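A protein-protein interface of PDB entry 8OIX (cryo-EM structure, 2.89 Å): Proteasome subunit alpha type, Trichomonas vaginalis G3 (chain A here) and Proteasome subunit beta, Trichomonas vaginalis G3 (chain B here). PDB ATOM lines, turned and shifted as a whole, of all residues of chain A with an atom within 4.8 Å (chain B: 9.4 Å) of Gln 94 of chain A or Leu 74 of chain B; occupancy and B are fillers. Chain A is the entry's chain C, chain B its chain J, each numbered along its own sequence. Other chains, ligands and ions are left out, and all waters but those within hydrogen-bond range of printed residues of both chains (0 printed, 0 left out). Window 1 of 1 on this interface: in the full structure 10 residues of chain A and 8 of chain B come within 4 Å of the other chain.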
ATOM      1  N   ILE A  67      33.935  -4.567  22.661  1.00  0.00           N
ATOM      2  CA  ILE A  67      33.388  -3.508  21.826  1.00  0.00           C
ATOM      3  C   ILE A  67      32.103  -4.001  21.185  1.00  0.00           C
ATOM      4  O   ILE A  67      31.156  -3.230  20.996  1.00  0.00           O
ATOM      5  CB  ILE A  67      34.396  -3.046  20.764  1.00  0.00           C
ATOM      6  CG1 ILE A  67      35.696  -2.627  21.437  1.00  0.00           C
ATOM      7  CG2 ILE A  67      33.818  -1.912  19.952  1.00  0.00           C
ATOM      8  CD1 ILE A  67      35.512  -1.599  22.524  1.00  0.00           C
ATOM      9  N   ASP A  68      32.058  -5.283  20.857  1.00  0.00           N
ATOM     10  CA  ASP A  68      30.845  -5.891  20.319  1.00  0.00           C
ATOM     11  C   ASP A  68      31.018  -7.401  20.404  1.00  0.00           C
ATOM     12  O   ASP A  68      32.098  -7.897  20.755  1.00  0.00           O
ATOM     13  CB  ASP A  68      30.577  -5.424  18.888  1.00  0.00           C
ATOM     14  CG  ASP A  68      29.118  -5.554  18.494  1.00  0.00           C
ATOM     15  OD1 ASP A  68      28.298  -5.908  19.366  1.00  0.00           O
ATOM     16  OD2 ASP A  68      28.790  -5.299  17.317  1.00  0.00           O
ATOM     17  N   ARG A  90      32.202   1.151  21.230  1.00  0.00           N
ATOM     18  CA  ARG A  90      30.952   0.415  21.374  1.00  0.00           C
ATOM     19  C   ARG A  90      29.809   1.162  20.708  1.00  0.00           C
ATOM     20  O   ARG A  90      28.997   0.562  19.991  1.00  0.00           O
ATOM     21  CB  ARG A  90      30.652   0.180  22.853  1.00  0.00           C
ATOM     22  CG  ARG A  90      31.590  -0.799  23.524  1.00  0.00           C
ATOM     23  CD  ARG A  90      31.426  -0.770  25.028  1.00  0.00           C
ATOM     24  NE  ARG A  90      32.217  -1.804  25.683  1.00  0.00           N
ATOM     25  CZ  ARG A  90      32.386  -1.896  26.994  1.00  0.00           C
ATOM     26  NH1 ARG A  90      31.850  -1.016  27.823  1.00  0.00           N
ATOM     27  NH2 ARG A  90      33.117  -2.891  27.485  1.00  0.00           N
ATOM     28  N   THR A  91      29.737   2.478  20.921  1.00  0.00           N
ATOM     29  CA  THR A  91      28.690   3.269  20.288  1.00  0.00           C
ATOM     30  C   THR A  91      28.818   3.235  18.771  1.00  0.00           C
ATOM     31  O   THR A  91      27.813   3.159  18.062  1.00  0.00           O
ATOM     32  CB  THR A  91      28.732   4.707  20.800  1.00  0.00           C
ATOM     33  OG1 THR A  91      28.802   4.702  22.231  1.00  0.00           O
ATOM     34  CG2 THR A  91      27.485   5.459  20.369  1.00  0.00           C
ATOM     35  N   SER A  92      30.049   3.260  18.254  1.00  0.00           N
ATOM     36  CA  SER A  92      30.245   3.237  16.806  1.00  0.00           C
ATOM     37  C   SER A  92      29.897   1.877  16.213  1.00  0.00           C
ATOM     38  O   SER A  92      29.280   1.800  15.145  1.00  0.00           O
ATOM     39  CB  SER A  92      31.685   3.615  16.469  1.00  0.00           C
ATOM     40  OG  SER A  92      32.001   4.900  16.972  1.00  0.00           O
ATOM     41  N   ALA A  93      30.292   0.794  16.885  1.00  0.00           N
ATOM     42  CA  ALA A  93      29.950  -0.542  16.410  1.00  0.00           C
ATOM     43  C   ALA A  93      28.444  -0.753  16.417  1.00  0.00           C
ATOM     44  O   ALA A  93      27.882  -1.321  15.474  1.00  0.00           O
ATOM     45  CB  ALA A  93      30.646  -1.600  17.263  1.00  0.00           C
ATOM     46  N   GLN A  94      27.767  -0.292  17.470  1.00  0.00           N
ATOM     47  CA  GLN A  94      26.320  -0.433  17.511  1.00  0.00           C
ATOM     48  C   GLN A  94      25.638   0.496  16.516  1.00  0.00           C
ATOM     49  O   GLN A  94      24.579   0.154  15.984  1.00  0.00           O
ATOM     50  CB  GLN A  94      25.811  -0.201  18.929  1.00  0.00           C
ATOM     51  CG  GLN A  94      26.331  -1.221  19.917  1.00  0.00           C
ATOM     52  CD  GLN A  94      26.103  -2.640  19.449  1.00  0.00           C
ATOM     53  OE1 GLN A  94      25.049  -2.967  18.904  1.00  0.00           O
ATOM     54  NE2 GLN A  94      27.092  -3.497  19.663  1.00  0.00           N
ATOM     55  N   LYS A  95      26.223   1.665  16.247  1.00  0.00           N
ATOM     56  CA  LYS A  95      25.711   2.532  15.192  1.00  0.00           C
ATOM     57  C   LYS A  95      25.811   1.852  13.835  1.00  0.00           C
ATOM     58  O   LYS A  95      24.880   1.918  13.024  1.00  0.00           O
ATOM     59  CB  LYS A  95      26.481   3.852  15.197  1.00  0.00           C
ATOM     60  CG  LYS A  95      26.395   4.651  13.911  1.00  0.00           C
ATOM     61  CD  LYS A  95      25.151   5.516  13.868  1.00  0.00           C
ATOM     62  CE  LYS A  95      25.176   6.430  12.658  1.00  0.00           C
ATOM     63  NZ  LYS A  95      26.384   7.301  12.657  1.00  0.00           N
ATOM     64  N   TYR A  96      26.929   1.170  13.579  1.00  0.00           N
ATOM     65  CA  TYR A  96      27.087   0.466  12.313  1.00  0.00           C
ATOM     66  C   TYR A  96      26.135  -0.717  12.229  1.00  0.00           C
ATOM     67  O   TYR A  96      25.621  -1.024  11.149  1.00  0.00           O
ATOM     68  CB  TYR A  96      28.530  -0.011  12.146  1.00  0.00           C
ATOM     69  CG  TYR A  96      28.819  -0.658  10.808  1.00  0.00           C
ATOM     70  CD1 TYR A  96      28.518  -1.993  10.575  1.00  0.00           C
ATOM     71  CD2 TYR A  96      29.424   0.058   9.787  1.00  0.00           C
ATOM     72  CE1 TYR A  96      28.782  -2.585   9.360  1.00  0.00           C
ATOM     73  CE2 TYR A  96      29.697  -0.528   8.569  1.00  0.00           C
ATOM     74  CZ  TYR A  96      29.374  -1.849   8.362  1.00  0.00           C
ATOM     75  OH  TYR A  96      29.646  -2.438   7.149  1.00  0.00           O
ATOM     76  N   LEU A  97      25.885  -1.383  13.357  1.00  0.00           N
ATOM     77  CA  LEU A  97      24.912  -2.468  13.376  1.00  0.00           C
ATOM     78  C   LEU A  97      23.506  -1.945  13.115  1.00  0.00           C
ATOM     79  O   LEU A  97      22.729  -2.571  12.389  1.00  0.00           O
ATOM     80  CB  LEU A  97      24.981  -3.205  14.713  1.00  0.00           C
ATOM     81  CG  LEU A  97      23.981  -4.335  14.954  1.00  0.00           C
ATOM     82  CD1 LEU A  97      24.032  -5.349  13.827  1.00  0.00           C
ATOM     83  CD2 LEU A  97      24.266  -5.003  16.285  1.00  0.00           C
ATOM     84  N   LYS A  98      23.157  -0.803  13.705  1.00  0.00           N
ATOM     85  CA  LYS A  98      21.846  -0.214  13.461  1.00  0.00           C
ATOM     86  C   LYS A  98      21.697   0.195  12.002  1.00  0.00           C
ATOM     87  O   LYS A  98      20.634   0.008  11.400  1.00  0.00           O
ATOM     88  CB  LYS A  98      21.637   0.990  14.379  1.00  0.00           C
ATOM     89  CG  LYS A  98      20.183   1.293  14.691  1.00  0.00           C
ATOM     90  CD  LYS A  98      19.989   2.747  15.078  1.00  0.00           C
ATOM     91  CE  LYS A  98      20.887   3.138  16.233  1.00  0.00           C
ATOM     92  NZ  LYS A  98      20.758   4.582  16.570  1.00  0.00           N
ATOM     93  N   ARG B  65      13.254  -1.904  16.599  1.00  0.00           N
ATOM     94  CA  ARG B  65      14.021  -3.101  16.914  1.00  0.00           C
ATOM     95  C   ARG B  65      15.515  -2.815  16.862  1.00  0.00           C
ATOM     96  O   ARG B  65      16.268  -3.231  17.749  1.00  0.00           O
ATOM     97  CB  ARG B  65      13.651  -4.219  15.941  1.00  0.00           C
ATOM     98  CG  ARG B  65      14.448  -5.506  16.094  1.00  0.00           C
ATOM     99  CD  ARG B  65      15.598  -5.633  15.100  1.00  0.00           C
ATOM    100  NE  ARG B  65      16.293  -6.914  15.200  1.00  0.00           N
ATOM    101  CZ  ARG B  65      16.953  -7.349  16.266  1.00  0.00           C
ATOM    102  NH1 ARG B  65      17.013  -6.643  17.384  1.00  0.00           N
ATOM    103  NH2 ARG B  65      17.566  -8.530  16.213  1.00  0.00           N
ATOM    104  N   GLU B  66      15.962  -2.082  15.841  1.00  0.00           N
ATOM    105  CA  GLU B  66      17.380  -1.766  15.717  1.00  0.00           C
ATOM    106  C   GLU B  66      17.822  -0.778  16.786  1.00  0.00           C
ATOM    107  O   GLU B  66      18.931  -0.888  17.319  1.00  0.00           O
ATOM    108  CB  GLU B  66      17.667  -1.222  14.321  1.00  0.00           C
ATOM    109  CG  GLU B  66      17.511  -2.257  13.226  1.00  0.00           C
ATOM    110  CD  GLU B  66      17.578  -1.650  11.843  1.00  0.00           C
ATOM    111  OE1 GLU B  66      17.733  -0.415  11.744  1.00  0.00           O
ATOM    112  OE2 GLU B  66      17.475  -2.408  10.857  1.00  0.00           O
ATOM    113  N   GLN B  67      16.962   0.181  17.135  1.00  0.00           N
ATOM    114  CA  GLN B  67      17.316   1.130  18.181  1.00  0.00           C
ATOM    115  C   GLN B  67      17.377   0.451  19.540  1.00  0.00           C
ATOM    116  O   GLN B  67      18.240   0.782  20.360  1.00  0.00           O
ATOM    117  CB  GLN B  67      16.318   2.285  18.204  1.00  0.00           C
ATOM    118  CG  GLN B  67      16.698   3.409  19.146  1.00  0.00           C
ATOM    119  CD  GLN B  67      18.008   4.069  18.764  1.00  0.00           C
ATOM    120  OE1 GLN B  67      18.133   4.653  17.688  1.00  0.00           O
ATOM    121  NE2 GLN B  67      18.991   3.984  19.651  1.00  0.00           N
ATOM    122  N   LEU B  68      16.541  -0.556  19.766  1.00  0.00           N
ATOM    123  CA  LEU B  68      16.580  -1.246  21.041  1.00  0.00           C
ATOM    124  C   LEU B  68      17.633  -2.334  21.056  1.00  0.00           C
ATOM    125  O   LEU B  68      18.104  -2.692  22.133  1.00  0.00           O
ATOM    126  CB  LEU B  68      15.216  -1.855  21.360  1.00  0.00           C
ATOM    127  CG  LEU B  68      14.113  -0.859  21.698  1.00  0.00           C
ATOM    128  CD1 LEU B  68      12.778  -1.554  21.637  1.00  0.00           C
ATOM    129  CD2 LEU B  68      14.349  -0.260  23.072  1.00  0.00           C
ATOM    130  N   ARG B  69      18.128  -2.739  19.892  1.00  0.00           N
ATOM    131  CA  ARG B  69      19.293  -3.603  19.848  1.00  0.00           C
ATOM    132  C   ARG B  69      20.560  -2.797  20.044  1.00  0.00           C
ATOM    133  O   ARG B  69      21.490  -3.268  20.698  1.00  0.00           O
ATOM    134  CB  ARG B  69      19.348  -4.350  18.510  1.00  0.00           C
ATOM    135  CG  ARG B  69      20.559  -5.238  18.313  1.00  0.00           C
ATOM    136  CD  ARG B  69      20.482  -5.934  16.968  1.00  0.00           C
ATOM    137  NE  ARG B  69      20.446  -4.967  15.879  1.00  0.00           N
ATOM    138  CZ  ARG B  69      20.378  -5.283  14.594  1.00  0.00           C
ATOM    139  NH1 ARG B  69      20.397  -6.542  14.191  1.00  0.00           N
ATOM    140  NH2 ARG B  69      20.301  -4.311  13.691  1.00  0.00           N
ATOM    141  N   PHE B  70      20.524  -1.529  19.639  1.00  0.00           N
ATOM    142  CA  PHE B  70      21.607  -0.594  19.900  1.00  0.00           C
ATOM    143  C   PHE B  70      21.685  -0.301  21.391  1.00  0.00           C
ATOM    144  O   PHE B  70      22.756  -0.421  22.000  1.00  0.00           O
ATOM    145  CB  PHE B  70      21.348   0.676  19.079  1.00  0.00           C
ATOM    146  CG  PHE B  70      22.317   1.801  19.314  1.00  0.00           C
ATOM    147  CD1 PHE B  70      22.134   2.693  20.357  1.00  0.00           C
ATOM    148  CD2 PHE B  70      23.371   2.009  18.447  1.00  0.00           C
ATOM    149  CE1 PHE B  70      23.009   3.740  20.552  1.00  0.00           C
ATOM    150  CE2 PHE B  70      24.255   3.051  18.642  1.00  0.00           C
ATOM    151  CZ  PHE B  70      24.073   3.917  19.695  1.00  0.00           C
ATOM    152  N   ASP B  71      20.531  -0.031  22.008  1.00  0.00           N
ATOM    153  CA  ASP B  71      20.507   0.284  23.431  1.00  0.00           C
ATOM    154  C   ASP B  71      20.832  -0.943  24.277  1.00  0.00           C
ATOM    155  O   ASP B  71      21.604  -0.847  25.236  1.00  0.00           O
ATOM    156  CB  ASP B  71      19.147   0.861  23.819  1.00  0.00           C
ATOM    157  CG  ASP B  71      18.775   2.079  23.000  1.00  0.00           C
ATOM    158  OD1 ASP B  71      19.580   2.489  22.141  1.00  0.00           O
ATOM    159  OD2 ASP B  71      17.671   2.626  23.210  1.00  0.00           O
ATOM    160  N   VAL B  72      20.273  -2.108  23.935  1.00  0.00           N
ATOM    161  CA  VAL B  72      20.506  -3.305  24.733  1.00  0.00           C
ATOM    162  C   VAL B  72      21.944  -3.782  24.584  1.00  0.00           C
ATOM    163  O   VAL B  72      22.577  -4.182  25.566  1.00  0.00           O
ATOM    164  CB  VAL B  72      19.500  -4.407  24.353  1.00  0.00           C
ATOM    165  CG1 VAL B  72      19.924  -5.737  24.927  1.00  0.00           C
ATOM    166  CG2 VAL B  72      18.127  -4.058  24.876  1.00  0.00           C
ATOM    167  N   ASN B  73      22.489  -3.754  23.364  1.00  0.00           N
ATOM    168  CA  ASN B  73      23.885  -4.124  23.184  1.00  0.00           C
ATOM    169  C   ASN B  73      24.810  -3.175  23.933  1.00  0.00           C
ATOM    170  O   ASN B  73      25.768  -3.621  24.572  1.00  0.00           O
ATOM    171  CB  ASN B  73      24.230  -4.167  21.700  1.00  0.00           C
ATOM    172  CG  ASN B  73      23.603  -5.350  20.990  1.00  0.00           C
ATOM    173  OD1 ASN B  73      22.941  -6.180  21.611  1.00  0.00           O
ATOM    174  ND2 ASN B  73      23.807  -5.430  19.681  1.00  0.00           N
ATOM    175  N   LEU B  74      24.543  -1.866  23.883  1.00  0.00           N
ATOM    176  CA  LEU B  74      25.382  -0.941  24.640  1.00  0.00           C
ATOM    177  C   LEU B  74      25.272  -1.192  26.138  1.00  0.00           C
ATOM    178  O   LEU B  74      26.280  -1.155  26.852  1.00  0.00           O
ATOM    179  CB  LEU B  74      25.028   0.507  24.311  1.00  0.00           C
ATOM    180  CG  LEU B  74      25.513   1.008  22.955  1.00  0.00           C
ATOM    181  CD1 LEU B  74      25.198   2.475  22.809  1.00  0.00           C
ATOM    182  CD2 LEU B  74      27.002   0.770  22.821  1.00  0.00           C
ATOM    183  N   LEU B  75      24.060  -1.447  26.634  1.00  0.00           N
ATOM    184  CA  LEU B  75      23.890  -1.719  28.057  1.00  0.00           C
ATOM    185  C   LEU B  75      24.628  -2.984  28.471  1.00  0.00           C
ATOM    186  O   LEU B  75      25.280  -3.015  29.520  1.00  0.00           O
ATOM    187  CB  LEU B  75      22.406  -1.826  28.396  1.00  0.00           C
ATOM    188  CG  LEU B  75      21.679  -0.487  28.490  1.00  0.00           C
ATOM    189  CD1 LEU B  75      20.177  -0.691  28.462  1.00  0.00           C
ATOM    190  CD2 LEU B  75      22.108   0.263  29.737  1.00  0.00           C
ATOM    191  N   GLU B  76      24.546  -4.037  27.657  1.00  0.00           N
ATOM    192  CA  GLU B  76      25.183  -5.296  28.023  1.00  0.00           C
ATOM    193  C   GLU B  76      26.698  -5.222  27.884  1.00  0.00           C
ATOM    194  O   GLU B  76      27.415  -5.921  28.604  1.00  0.00           O
ATOM    195  CB  GLU B  76      24.624  -6.439  27.178  1.00  0.00           C
ATOM    196  CG  GLU B  76      23.149  -6.714  27.416  1.00  0.00           C
ATOM    197  CD  GLU B  76      22.598  -7.770  26.486  1.00  0.00           C
ATOM    198  OE1 GLU B  76      23.389  -8.357  25.718  1.00  0.00           O
ATOM    199  OE2 GLU B  76      21.378  -8.026  26.532  1.00  0.00           O
ATOM    200  N   LEU B  77      27.201  -4.396  26.966  1.00  0.00           N
ATOM    201  CA  LEU B  77      28.639  -4.175  26.890  1.00  0.00           C
ATOM    202  C   LEU B  77      29.132  -3.371  28.086  1.00  0.00           C
ATOM    203  O   LEU B  77      30.127  -3.734  28.725  1.00  0.00           O
ATOM    204  CB  LEU B  77      28.990  -3.471  25.581  1.00  0.00           C
ATOM    205  CG  LEU B  77      28.805  -4.305  24.315  1.00  0.00           C
ATOM    206  CD1 LEU B  77      28.822  -3.413  23.091  1.00  0.00           C
ATOM    207  CD2 LEU B  77      29.879  -5.370  24.220  1.00  0.00           C
ATOM    208  N   ARG B  78      28.445  -2.274  28.407  1.00  0.00           N
ATOM    209  CA  ARG B  78      28.874  -1.408  29.496  1.00  0.00           C
ATOM    210  C   ARG B  78      28.625  -2.024  30.865  1.00  0.00           C
ATOM    211  O   ARG B  78      29.204  -1.559  31.851  1.00  0.00           O
ATOM    212  CB  ARG B  78      28.168  -0.056  29.388  1.00  0.00           C
ATOM    213  CG  ARG B  78      28.537   0.720  28.135  1.00  0.00           C
ATOM    214  CD  ARG B  78      27.824   2.058  28.057  1.00  0.00           C
ATOM    215  NE  ARG B  78      26.391   1.905  27.838  1.00  0.00           N
ATOM    216  CZ  ARG B  78      25.611   2.836  27.303  1.00  0.00           C
ATOM    217  NH1 ARG B  78      26.099   3.997  26.901  1.00  0.00           N
ATOM    218  NH2 ARG B  78      24.312   2.592  27.165  1.00  0.00           N
ATOM    219  N   GLU B  79      27.798  -3.064  30.950  1.00  0.00           N
ATOM    220  CA  GLU B  79      27.458  -3.671  32.226  1.00  0.00           C
ATOM    221  C   GLU B  79      27.817  -5.145  32.313  1.00  0.00           C
ATOM    222  O   GLU B  79      27.634  -5.744  33.379  1.00  0.00           O
ATOM    223  CB  GLU B  79      25.960  -3.504  32.511  1.00  0.00           C
ATOM    224  CG  GLU B  79      25.497  -2.065  32.543  1.00  0.00           C
ATOM    225  CD  GLU B  79      24.020  -1.938  32.828  1.00  0.00           C
ATOM    226  OE1 GLU B  79      23.435  -2.898  33.373  1.00  0.00           O
ATOM    227  OE2 GLU B  79      23.441  -0.878  32.512  1.00  0.00           O
ATOM    228  N   GLU B  80      28.313  -5.747  31.232  1.00  0.00           N
ATOM    229  CA  GLU B  80      28.745  -7.143  31.209  1.00  0.00           C
ATOM    230  C   GLU B  80      27.643  -8.098  31.662  1.00  0.00           C
ATOM    231  O   GLU B  80      27.924  -9.236  32.049  1.00  0.00           O
ATOM    232  CB  GLU B  80      30.001  -7.347  32.064  1.00  0.00           C
ATOM    233  CG  GLU B  80      31.152  -6.410  31.724  1.00  0.00           C
ATOM    234  CD  GLU B  80      32.036  -6.935  30.606  1.00  0.00           C
ATOM    235  OE1 GLU B  80      31.500  -7.452  29.604  1.00  0.00           O
ATOM    236  OE2 GLU B  80      33.273  -6.831  30.734  1.00  0.00           O
ATOM    237  N   ARG B  81      26.388  -7.652  31.618  1.00  0.00           N
ATOM    238  CA  ARG B  81      25.261  -8.422  32.108  1.00  0.00           C
ATOM    239  C   ARG B  81      24.101  -8.304  31.130  1.00  0.00           C
ATOM    240  O   ARG B  81      23.893  -7.231  30.543  1.00  0.00           O
ATOM    241  CB  ARG B  81      24.827  -7.925  33.494  1.00  0.00           C
ATOM    242  CG  ARG B  81      24.031  -8.925  34.303  1.00  0.00           C
ATOM    243  CD  ARG B  81      24.183  -8.655  35.789  1.00  0.00           C
ATOM    244  NE  ARG B  81      25.585  -8.638  36.195  1.00  0.00           N
ATOM    245  CZ  ARG B  81      26.359  -9.711  36.290  1.00  0.00           C
ATOM    246  NH1 ARG B  81      25.901 -10.922  36.019  1.00  0.00           N
ATOM    247  NH2 ARG B  81      27.626  -9.565  36.665  1.00  0.00           N
ATOM    248  N   ILE B  83      20.298  -7.730  29.882  1.00  0.00           N
ATOM    249  CA  ILE B  83      19.287  -6.785  30.343  1.00  0.00           C
ATOM    250  C   ILE B  83      18.102  -7.549  30.919  1.00  0.00           C
ATOM    251  O   ILE B  83      17.720  -8.614  30.417  1.00  0.00           O
ATOM    252  CB  ILE B  83      18.868  -5.844  29.198  1.00  0.00           C
ATOM    253  CG1 ILE B  83      18.116  -4.632  29.747  1.00  0.00           C
ATOM    254  CG2 ILE B  83      18.039  -6.577  28.153  1.00  0.00           C
ATOM    255  CD1 ILE B  83      17.887  -3.550  28.725  1.00  0.00           C
ATOM    256  N   LEU B  91      13.459   0.495  29.178  1.00  0.00           N
ATOM    257  CA  LEU B  91      14.226   0.965  28.029  1.00  0.00           C
ATOM    258  C   LEU B  91      13.322   1.232  26.833  1.00  0.00           C
ATOM    259  O   LEU B  91      13.474   2.248  26.147  1.00  0.00           O
ATOM    260  CB  LEU B  91      15.301  -0.057  27.670  1.00  0.00           C
ATOM    261  CG  LEU B  91      16.123   0.235  26.419  1.00  0.00           C
ATOM    262  CD1 LEU B  91      16.840   1.564  26.558  1.00  0.00           C
ATOM    263  CD2 LEU B  91      17.109  -0.885  26.189  1.00  0.00           C
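The backbone carbonyl oxygen of Leu 77 of chain B sits at hydrogen-bond distance from the guanidinium group of Arg 90 of chain A, at 3.3 Å.
O of Lys 98 of chain A lies close to OE1 of Glu 66 of chain B (3.0 Å).
The guanidinium group (NH2) of Arg 69 of chain B lies within hydrogen-bond range of the backbone carbonyl oxygen (O) of Leu 97 of chain A.
The side-chain amide nitrogen (ND2) of Asn 73 of chain B lies within hydrogen-bond range of the side-chain amide oxygen (OE1) of Gln 94 of chain A (2.9 Å).
OE1 of Gln 67 of chain B lies within hydrogen-bond range of NZ of Lys 98 of chain A, at 2.9 Å.
The side-chain amide nitrogen (ND2) of Asn 73 of chain B sits close to the backbone carbonyl oxygen (O) of Arg 69 of chain B (3.3 Å).
The side-chain amide nitrogen (NE2) of Gln 94 of chain A sits at hydrogen-bond distance from the side-chain carboxylate (OD1) of Asp 68 of chain A (2.7 Å).
The side-chain amide nitrogen (NE2) of Gln 67 of chain B is in hydrogen-bond range of the side-chain carboxylate (OD1) of Asp 71 of chain B.
The backbone carbonyl oxygen of Leu 74 of chain B sits close to the guanidinium group of Arg 78 of chain B, 3.2 Å away.
Among the printed residues, pairs that only touch across the chains: Ile 67 of chain A with Leu 77 of chain B (3.1 Å), Arg 90 of chain A with Leu 74 of chain B (3.5 Å), Arg 90 of chain A with Arg 78 of chain B (3.4 Å), Thr 91 of chain A with Phe 70 of chain B (3.6 Å), Thr 91 of chain A with Leu 74 of chain B (3.7 Å), Gln 94 of chain A with Arg 69 of chain B (3.997 Å), Gln 94 of chain A with Phe 70 of chain B (3.3 Å), Gln 94 of chain A with Leu 74 of chain B (3.6 Å), Gln 94 of chain A with Leu 77 of chain B (3.8 Å), Lys 95 of chain A with Phe 70 of chain B (3.4 Å), Leu 97 of chain A with Asn 73 of chain B (3.5 Å) and Lys 98 of chain A with Phe 70 of chain B (3.5 Å).
Of the printed residues of chain B, Gln 94 of chain A touches Arg 69, Phe 70, Asn 73, Leu 74 and Leu 77.
Leu 74 of chain B touches three residues of chain A.
Of the printed residues of chain A, Asn 73 of chain B touches Gln 94 and Leu 97.
Of the printed residues of chain A, Gln 67 of chain B touches Lys 98 (2.9 Å).
Printed residues of chain B within 4 Å of Arg 90 of chain A: Leu 74 (3.5 Å), Leu 77 (3.3 Å) and Arg 78 (3.4 Å).
Ile 83 of chain B touches none of the printed residues of chain A.
Glu 76 of chain B touches none of the printed residues of chain A.
The nearest printed residue of chain A that does not touch Arg 78 of chain B is Thr 91 of chain A (5.4 Å).
Printed residues of chain A that touch a printed residue of chain B: Ile 67, Arg 90, Thr 91, Gln 94, Lys 95, Leu 97 and Lys 98.
Hydrophobic or aromatic side chains of chain A within 4 Å of the printed part of chain B: Leu 97.
Along chain B the printed residues that touch a printed residue of chain A span positions 66 to 78.
Among the printed residues, no Asp or Glu carboxylate lies within 4 Å of a Lys or Arg side-chain nitrogen of the other chain.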
